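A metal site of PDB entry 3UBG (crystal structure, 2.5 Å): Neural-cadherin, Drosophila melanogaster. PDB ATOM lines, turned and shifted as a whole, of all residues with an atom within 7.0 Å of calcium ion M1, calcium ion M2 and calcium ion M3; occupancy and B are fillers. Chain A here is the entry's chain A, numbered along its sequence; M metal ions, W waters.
Calcium ion M2 is bound by the side-chain carboxylate (OD1) of Asp 98 (2.4 Å), the backbone carbonyl oxygen (O) of Val 99 (2.4 Å), the side-chain carboxylate (OD1) of Asp 136 (2.5 Å), the side-chain carboxylate (OD1) of Asp 101 (2.5 Å), the side-chain carboxylate (OE1) of Glu 13 (2.6 Å), the side-chain carboxylate (OE2) of Glu 61 (2.6 Å) and the side-chain carboxylate (OE1) of Glu 61 (2.7 Å).
Calcium ion M3 is bound by the side-chain carboxylate (OE2) of Glu 102 (2.5 Å), the side-chain carboxylate (OE1) of Glu 61 (2.5 Å), the side-chain carboxylate (OE2) of Glu 13 (2.5 Å), the side-chain carboxylate (OD1) of Asp 59 (2.5 Å), the side-chain carboxylate (OD2) of Asp 101 (2.6 Å), water W1 (2.7 Å) and the side-chain carboxylate (OD1) of Asp 101 (2.8 Å).
Calcium ion M3 has seven donor atoms within binding distance.
Calcium ion M1 is bound by the backbone carbonyl oxygen (O) of Glu 102 (2.4 Å).
OD2 of Asp 136 binds calcium ion M1 (2.4 Å).
Calcium ion M1 is bound by OD2 of Asp 185.
Calcium ion M1 is bound by OD2 of Asp 134.
The side-chain amide oxygen (OD1) of Asn 100 is bound to calcium ion M1 (2.5 Å).
OD1 of Asp 134 binds calcium ion M1, 2.6 Å away.
Calcium ion M1 is bound by the side-chain amide oxygen (OE1) of Gln 196 (2.6 Å).
Calcium ion M1 has seven donor atoms within binding distance.
OG1 of Thr 137 is in hydrogen-bond range of OD2 of Asp 98, at 3.0 Å.
The backbone NH (N) of Asn 187 is in hydrogen-bond range of the side-chain carboxylate (OD1) of Asp 185, 2.9 Å away.
The side-chain carboxylate (OD1) of Asp 185 sits at hydrogen-bond distance from the backbone NH (N) of Asn 140 (2.9 Å).
The backbone carbonyl oxygen of Asp 138 sits at hydrogen-bond distance from the side-chain amide nitrogen of Asn 100.
OE2 of Glu 13 sits close to N of Tyr 60 (2.6 Å).
O of Lys 97 sits at hydrogen-bond distance from N of Glu 13 (2.9 Å).
The backbone NH (N) of Gln 196 is in hydrogen-bond range of the backbone carbonyl oxygen (O) of Gly 188.
Of the 25 residues printed, 5 come within 4 Å of calcium ion M3.
The nearest printed residue that does not touch calcium ion M3 is Tyr 60 (4.1 Å).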
ATOM      1  N   GLU A  13      -7.957 -21.990  22.237  1.00  0.00           N
ATOM      2  CA  GLU A  13      -9.093 -22.756  21.723  1.00  0.00           C
ATOM      3  C   GLU A  13      -9.268 -22.519  20.219  1.00  0.00           C
ATOM      4  O   GLU A  13      -9.784 -23.379  19.489  1.00  0.00           O
ATOM      5  CB  GLU A  13     -10.370 -22.418  22.480  1.00  0.00           C
ATOM      6  CG  GLU A  13     -10.825 -20.983  22.306  1.00  0.00           C
ATOM      7  CD  GLU A  13     -12.020 -20.610  23.173  1.00  0.00           C
ATOM      8  OE1 GLU A  13     -12.039 -19.472  23.662  1.00  0.00           O
ATOM      9  OE2 GLU A  13     -12.933 -21.449  23.377  1.00  0.00           O
ATOM     10  N   TRP A  58     -12.334 -27.098  19.408  1.00  0.00           N
ATOM     11  CA  TRP A  58     -11.979 -26.787  20.764  1.00  0.00           C
ATOM     12  C   TRP A  58     -12.839 -25.655  21.292  1.00  0.00           C
ATOM     13  O   TRP A  58     -13.198 -24.741  20.541  1.00  0.00           O
ATOM     14  CB  TRP A  58     -10.488 -26.477  20.847  1.00  0.00           C
ATOM     15  CG  TRP A  58      -9.630 -27.718  20.684  1.00  0.00           C
ATOM     16  CD1 TRP A  58     -10.071 -29.006  20.539  1.00  0.00           C
ATOM     17  CD2 TRP A  58      -8.207 -27.773  20.621  1.00  0.00           C
ATOM     18  NE1 TRP A  58      -9.005 -29.863  20.421  1.00  0.00           N
ATOM     19  CE2 TRP A  58      -7.846 -29.134  20.466  1.00  0.00           C
ATOM     20  CE3 TRP A  58      -7.199 -26.805  20.702  1.00  0.00           C
ATOM     21  CZ2 TRP A  58      -6.506 -29.547  20.391  1.00  0.00           C
ATOM     22  CZ3 TRP A  58      -5.854 -27.225  20.621  1.00  0.00           C
ATOM     23  CH2 TRP A  58      -5.527 -28.585  20.473  1.00  0.00           C
ATOM     24  N   ASP A  59     -13.180 -25.724  22.577  1.00  0.00           N
ATOM     25  CA  ASP A  59     -14.062 -24.756  23.191  1.00  0.00           C
ATOM     26  C   ASP A  59     -13.733 -24.622  24.678  1.00  0.00           C
ATOM     27  O   ASP A  59     -14.094 -25.473  25.497  1.00  0.00           O
ATOM     28  CB  ASP A  59     -15.531 -25.130  22.958  1.00  0.00           C
ATOM     29  CG  ASP A  59     -16.522 -24.145  23.587  1.00  0.00           C
ATOM     30  OD1 ASP A  59     -16.134 -23.032  23.994  1.00  0.00           O
ATOM     31  OD2 ASP A  59     -17.705 -24.509  23.668  1.00  0.00           O
ATOM     32  N   TYR A  60     -13.023 -23.535  24.990  1.00  0.00           N
ATOM     33  CA  TYR A  60     -12.594 -23.205  26.329  1.00  0.00           C
ATOM     34  C   TYR A  60     -13.790 -23.128  27.296  1.00  0.00           C
ATOM     35  O   TYR A  60     -13.696 -23.545  28.448  1.00  0.00           O
ATOM     36  CB  TYR A  60     -11.850 -21.869  26.277  1.00  0.00           C
ATOM     37  CG  TYR A  60     -11.317 -21.395  27.617  1.00  0.00           C
ATOM     38  CD1 TYR A  60     -10.034 -21.700  28.043  1.00  0.00           C
ATOM     39  CD2 TYR A  60     -12.119 -20.611  28.454  1.00  0.00           C
ATOM     40  CE1 TYR A  60      -9.553 -21.255  29.272  1.00  0.00           C
ATOM     41  CE2 TYR A  60     -11.661 -20.176  29.661  1.00  0.00           C
ATOM     42  CZ  TYR A  60     -10.390 -20.502  30.083  1.00  0.00           C
ATOM     43  OH  TYR A  60      -9.962 -20.032  31.313  1.00  0.00           O
ATOM     44  N   GLU A  61     -14.925 -22.617  26.819  1.00  0.00           N
ATOM     45  CA  GLU A  61     -16.139 -22.577  27.609  1.00  0.00           C
ATOM     46  C   GLU A  61     -16.680 -23.960  28.009  1.00  0.00           C
ATOM     47  O   GLU A  61     -17.255 -24.101  29.077  1.00  0.00           O
ATOM     48  CB  GLU A  61     -17.226 -21.740  26.913  1.00  0.00           C
ATOM     49  CG  GLU A  61     -16.978 -20.242  26.973  1.00  0.00           C
ATOM     50  CD  GLU A  61     -15.690 -19.798  26.282  1.00  0.00           C
ATOM     51  OE1 GLU A  61     -15.401 -20.300  25.167  1.00  0.00           O
ATOM     52  OE2 GLU A  61     -14.949 -18.953  26.844  1.00  0.00           O
ATOM     53  N   GLU A  62     -16.504 -24.979  27.197  1.00  0.00           N
ATOM     54  CA  GLU A  62     -16.981 -26.288  27.614  1.00  0.00           C
ATOM     55  C   GLU A  62     -16.000 -27.141  28.434  1.00  0.00           C
ATOM     56  O   GLU A  62     -16.386 -28.168  28.974  1.00  0.00           O
ATOM     57  CB  GLU A  62     -17.528 -27.099  26.427  1.00  0.00           C
ATOM     58  CG  GLU A  62     -18.798 -26.516  25.796  1.00  0.00           C
ATOM     59  CD  GLU A  62     -19.774 -25.971  26.823  1.00  0.00           C
ATOM     60  OE1 GLU A  62     -20.025 -26.657  27.845  1.00  0.00           O
ATOM     61  OE2 GLU A  62     -20.284 -24.843  26.617  1.00  0.00           O
ATOM     62  N   LYS A  97      -6.303 -22.175  25.961  1.00  0.00           N
ATOM     63  CA  LYS A  97      -6.355 -20.771  26.307  1.00  0.00           C
ATOM     64  C   LYS A  97      -7.589 -20.102  25.725  1.00  0.00           C
ATOM     65  O   LYS A  97      -7.968 -20.371  24.593  1.00  0.00           O
ATOM     66  CB  LYS A  97      -5.084 -20.084  25.819  1.00  0.00           C
ATOM     67  CG  LYS A  97      -3.895 -20.410  26.692  1.00  0.00           C
ATOM     68  CD  LYS A  97      -2.678 -19.713  26.203  1.00  0.00           C
ATOM     69  CE  LYS A  97      -2.092 -20.453  25.045  1.00  0.00           C
ATOM     70  NZ  LYS A  97      -0.935 -19.739  24.490  1.00  0.00           N
ATOM     71  N   ASP A  98      -8.209 -19.244  26.514  1.00  0.00           N
ATOM     72  CA  ASP A  98      -9.442 -18.602  26.117  1.00  0.00           C
ATOM     73  C   ASP A  98      -9.206 -17.534  25.054  1.00  0.00           C
ATOM     74  O   ASP A  98      -8.270 -16.749  25.153  1.00  0.00           O
ATOM     75  CB  ASP A  98     -10.110 -17.941  27.319  1.00  0.00           C
ATOM     76  CG  ASP A  98     -11.394 -17.243  26.955  1.00  0.00           C
ATOM     77  OD1 ASP A  98     -12.205 -17.887  26.279  1.00  0.00           O
ATOM     78  OD2 ASP A  98     -11.585 -16.061  27.312  1.00  0.00           O
ATOM     79  N   VAL A  99     -10.082 -17.508  24.052  1.00  0.00           N
ATOM     80  CA  VAL A  99     -10.117 -16.469  23.052  1.00  0.00           C
ATOM     81  C   VAL A  99     -11.525 -15.866  23.111  1.00  0.00           C
ATOM     82  O   VAL A  99     -12.468 -16.518  23.523  1.00  0.00           O
ATOM     83  CB  VAL A  99      -9.778 -17.049  21.638  1.00  0.00           C
ATOM     84  CG1 VAL A  99     -10.161 -16.084  20.555  1.00  0.00           C
ATOM     85  CG2 VAL A  99      -8.286 -17.393  21.516  1.00  0.00           C
ATOM     86  N   ASN A 100     -11.682 -14.609  22.741  1.00  0.00           N
ATOM     87  CA  ASN A 100     -13.003 -14.014  22.825  1.00  0.00           C
ATOM     88  C   ASN A 100     -13.822 -14.416  21.608  1.00  0.00           C
ATOM     89  O   ASN A 100     -13.656 -13.855  20.526  1.00  0.00           O
ATOM     90  CB  ASN A 100     -12.898 -12.493  22.936  1.00  0.00           C
ATOM     91  CG  ASN A 100     -14.182 -11.850  23.441  1.00  0.00           C
ATOM     92  OD1 ASN A 100     -15.274 -12.217  23.031  1.00  0.00           O
ATOM     93  ND2 ASN A 100     -14.048 -10.858  24.302  1.00  0.00           N
ATOM     94  N   ASP A 101     -14.702 -15.389  21.786  1.00  0.00           N
ATOM     95  CA  ASP A 101     -15.317 -16.051  20.651  1.00  0.00           C
ATOM     96  C   ASP A 101     -16.755 -16.494  20.915  1.00  0.00           C
ATOM     97  O   ASP A 101     -17.324 -17.260  20.139  1.00  0.00           O
ATOM     98  CB  ASP A 101     -14.468 -17.251  20.226  1.00  0.00           C
ATOM     99  CG  ASP A 101     -14.576 -18.421  21.181  1.00  0.00           C
ATOM    100  OD1 ASP A 101     -14.949 -18.205  22.354  1.00  0.00           O
ATOM    101  OD2 ASP A 101     -14.281 -19.567  20.779  1.00  0.00           O
ATOM    102  N   GLU A 102     -17.330 -16.040  22.017  1.00  0.00           N
ATOM    103  CA  GLU A 102     -18.727 -16.353  22.317  1.00  0.00           C
ATOM    104  C   GLU A 102     -19.574 -15.091  22.414  1.00  0.00           C
ATOM    105  O   GLU A 102     -19.171 -14.098  23.005  1.00  0.00           O
ATOM    106  CB  GLU A 102     -18.835 -17.173  23.605  1.00  0.00           C
ATOM    107  CG  GLU A 102     -18.004 -18.450  23.581  1.00  0.00           C
ATOM    108  CD  GLU A 102     -18.401 -19.387  22.451  1.00  0.00           C
ATOM    109  OE1 GLU A 102     -19.458 -19.177  21.815  1.00  0.00           O
ATOM    110  OE2 GLU A 102     -17.678 -20.356  22.195  1.00  0.00           O
ATOM    111  N   PRO A 103     -20.761 -15.098  21.808  1.00  0.00           N
ATOM    112  CA  PRO A 103     -21.586 -13.888  21.844  1.00  0.00           C
ATOM    113  C   PRO A 103     -22.173 -13.621  23.236  1.00  0.00           C
ATOM    114  O   PRO A 103     -22.345 -14.563  24.016  1.00  0.00           O
ATOM    115  CB  PRO A 103     -22.697 -14.205  20.832  1.00  0.00           C
ATOM    116  CG  PRO A 103     -22.811 -15.710  20.850  1.00  0.00           C
ATOM    117  CD  PRO A 103     -21.393 -16.200  21.060  1.00  0.00           C
ATOM    118  N   PRO A 104     -22.469 -12.345  23.557  1.00  0.00           N
ATOM    119  CA  PRO A 104     -23.187 -12.012  24.790  1.00  0.00           C
ATOM    120  C   PRO A 104     -24.673 -12.362  24.740  1.00  0.00           C
ATOM    121  O   PRO A 104     -25.238 -12.557  23.669  1.00  0.00           O
ATOM    122  CB  PRO A 104     -23.040 -10.498  24.872  1.00  0.00           C
ATOM    123  CG  PRO A 104     -22.937 -10.075  23.439  1.00  0.00           C
ATOM    124  CD  PRO A 104     -22.091 -11.138  22.805  1.00  0.00           C
ATOM    125  N   ASP A 134     -21.538 -12.228  29.144  1.00  0.00           N
ATOM    126  CA  ASP A 134     -20.766 -12.769  28.040  1.00  0.00           C
ATOM    127  C   ASP A 134     -19.813 -13.827  28.595  1.00  0.00           C
ATOM    128  O   ASP A 134     -19.190 -13.616  29.623  1.00  0.00           O
ATOM    129  CB  ASP A 134     -19.994 -11.652  27.355  1.00  0.00           C
ATOM    130  CG  ASP A 134     -19.199 -12.144  26.176  1.00  0.00           C
ATOM    131  OD1 ASP A 134     -18.199 -12.895  26.364  1.00  0.00           O
ATOM    132  OD2 ASP A 134     -19.594 -11.765  25.058  1.00  0.00           O
ATOM    133  N   PRO A 135     -19.697 -14.971  27.914  1.00  0.00           N
ATOM    134  CA  PRO A 135     -19.000 -16.153  28.413  1.00  0.00           C
ATOM    135  C   PRO A 135     -17.486 -16.017  28.459  1.00  0.00           C
ATOM    136  O   PRO A 135     -16.858 -16.718  29.223  1.00  0.00           O
ATOM    137  CB  PRO A 135     -19.399 -17.254  27.419  1.00  0.00           C
ATOM    138  CG  PRO A 135     -20.585 -16.713  26.679  1.00  0.00           C
ATOM    139  CD  PRO A 135     -20.394 -15.237  26.634  1.00  0.00           C
ATOM    140  N   ASP A 136     -16.897 -15.125  27.683  1.00  0.00           N
ATOM    141  CA  ASP A 136     -15.441 -15.049  27.650  1.00  0.00           C
ATOM    142  C   ASP A 136     -14.873 -14.390  28.908  1.00  0.00           C
ATOM    143  O   ASP A 136     -15.588 -13.697  29.625  1.00  0.00           O
ATOM    144  CB  ASP A 136     -14.987 -14.346  26.373  1.00  0.00           C
ATOM    145  CG  ASP A 136     -15.558 -15.022  25.131  1.00  0.00           C
ATOM    146  OD1 ASP A 136     -15.608 -16.245  25.081  1.00  0.00           O
ATOM    147  OD2 ASP A 136     -16.006 -14.340  24.204  1.00  0.00           O
ATOM    148  N   THR A 137     -13.598 -14.637  29.191  1.00  0.00           N
ATOM    149  CA  THR A 137     -12.945 -14.029  30.351  1.00  0.00           C
ATOM    150  C   THR A 137     -12.645 -12.561  30.058  1.00  0.00           C
ATOM    151  O   THR A 137     -12.367 -11.794  30.966  1.00  0.00           O
ATOM    152  CB  THR A 137     -11.611 -14.742  30.703  1.00  0.00           C
ATOM    153  OG1 THR A 137     -10.631 -14.511  29.676  1.00  0.00           O
ATOM    154  CG2 THR A 137     -11.803 -16.245  30.862  1.00  0.00           C
ATOM    155  N   ASP A 138     -12.762 -12.180  28.793  1.00  0.00           N
ATOM    156  CA  ASP A 138     -12.206 -10.948  28.252  1.00  0.00           C
ATOM    157  C   ASP A 138     -13.278 -10.014  27.643  1.00  0.00           C
ATOM    158  O   ASP A 138     -13.016  -9.291  26.674  1.00  0.00           O
ATOM    159  CB  ASP A 138     -11.192 -11.362  27.190  1.00  0.00           C
ATOM    160  CG  ASP A 138     -10.506 -10.181  26.533  1.00  0.00           C
ATOM    161  OD1 ASP A 138     -10.419  -9.096  27.151  1.00  0.00           O
ATOM    162  OD2 ASP A 138     -10.022 -10.368  25.379  1.00  0.00           O
ATOM    163  N   HIS A 139     -14.474 -10.015  28.203  1.00  0.00           N
ATOM    164  CA  HIS A 139     -15.590  -9.258  27.612  1.00  0.00           C
ATOM    165  C   HIS A 139     -15.561  -7.757  27.874  1.00  0.00           C
ATOM    166  O   HIS A 139     -14.893  -7.263  28.767  1.00  0.00           O
ATOM    167  CB  HIS A 139     -16.900  -9.806  28.149  1.00  0.00           C
ATOM    168  CG  HIS A 139     -16.965  -9.830  29.633  1.00  0.00           C
ATOM    169  ND1 HIS A 139     -17.203  -8.709  30.381  1.00  0.00           N
ATOM    170  CD2 HIS A 139     -16.795 -10.849  30.509  1.00  0.00           C
ATOM    171  CE1 HIS A 139     -17.192  -9.029  31.665  1.00  0.00           C
ATOM    172  NE2 HIS A 139     -16.954 -10.325  31.767  1.00  0.00           N
ATOM    173  N   ASN A 140     -16.321  -7.030  27.064  1.00  0.00           N
ATOM    174  CA  ASN A 140     -16.423  -5.582  27.149  1.00  0.00           C
ATOM    175  C   ASN A 140     -17.770  -5.145  26.591  1.00  0.00           C
ATOM    176  O   ASN A 140     -17.877  -4.803  25.412  1.00  0.00           O
ATOM    177  CB  ASN A 140     -15.278  -4.943  26.361  1.00  0.00           C
ATOM    178  CG  ASN A 140     -15.331  -3.417  26.362  1.00  0.00           C
ATOM    179  OD1 ASN A 140     -15.788  -2.791  27.322  1.00  0.00           O
ATOM    180  ND2 ASN A 140     -14.840  -2.815  25.280  1.00  0.00           N
ATOM    181  N   ASP A 185     -20.347  -7.319  22.640  1.00  0.00           N
ATOM    182  CA  ASP A 185     -19.061  -7.464  23.293  1.00  0.00           C
ATOM    183  C   ASP A 185     -18.058  -6.815  22.351  1.00  0.00           C
ATOM    184  O   ASP A 185     -17.729  -7.376  21.301  1.00  0.00           O
ATOM    185  CB  ASP A 185     -18.722  -8.933  23.570  1.00  0.00           C
ATOM    186  CG  ASP A 185     -17.309  -9.116  24.126  1.00  0.00           C
ATOM    187  OD1 ASP A 185     -16.639  -8.105  24.425  1.00  0.00           O
ATOM    188  OD2 ASP A 185     -16.878 -10.279  24.294  1.00  0.00           O
ATOM    189  N   ASN A 187     -15.056  -6.484  22.626  1.00  0.00           N
ATOM    190  CA  ASN A 187     -13.771  -7.167  22.581  1.00  0.00           C
ATOM    191  C   ASN A 187     -13.744  -8.365  21.635  1.00  0.00           C
ATOM    192  O   ASN A 187     -12.744  -9.070  21.581  1.00  0.00           O
ATOM    193  CB  ASN A 187     -13.354  -7.632  23.970  1.00  0.00           C
ATOM    194  CG  ASN A 187     -12.648  -6.558  24.737  1.00  0.00           C
ATOM    195  OD1 ASN A 187     -12.543  -5.419  24.278  1.00  0.00           O
ATOM    196  ND2 ASN A 187     -12.167  -6.898  25.931  1.00  0.00           N
ATOM    197  N   GLY A 188     -14.837  -8.592  20.910  1.00  0.00           N
ATOM    198  CA  GLY A 188     -14.937  -9.755  20.031  1.00  0.00           C
ATOM    199  C   GLY A 188     -15.479  -9.414  18.653  1.00  0.00           C
ATOM    200  O   GLY A 188     -16.690  -9.210  18.486  1.00  0.00           O
ATOM    201  N   GLN A 196     -19.553  -9.236  18.156  1.00  0.00           N
ATOM    202  CA  GLN A 196     -20.495 -10.202  18.707  1.00  0.00           C
ATOM    203  C   GLN A 196     -21.680  -9.514  19.406  1.00  0.00           C
ATOM    204  O   GLN A 196     -21.505  -8.529  20.121  1.00  0.00           O
ATOM    205  CB  GLN A 196     -19.821 -11.123  19.709  1.00  0.00           C
ATOM    206  CG  GLN A 196     -18.597 -11.842  19.211  1.00  0.00           C
ATOM    207  CD  GLN A 196     -17.651 -12.129  20.362  1.00  0.00           C
ATOM    208  OE1 GLN A 196     -17.825 -11.609  21.460  1.00  0.00           O
ATOM    209  NE2 GLN A 196     -16.639 -12.942  20.117  1.00  0.00           N
HETATM  210 CA    CA M   1     -17.588 -12.572  23.882  1.00  0.00          CA
HETATM  211 CA    CA M   2     -13.909 -18.048  24.660  1.00  0.00          CA
HETATM  212 CA    CA M   3     -15.341 -20.968  22.748  1.00  0.00          CA
HETATM  213  O   HOH W   1     -15.227 -22.802  20.703  1.00  0.00           O
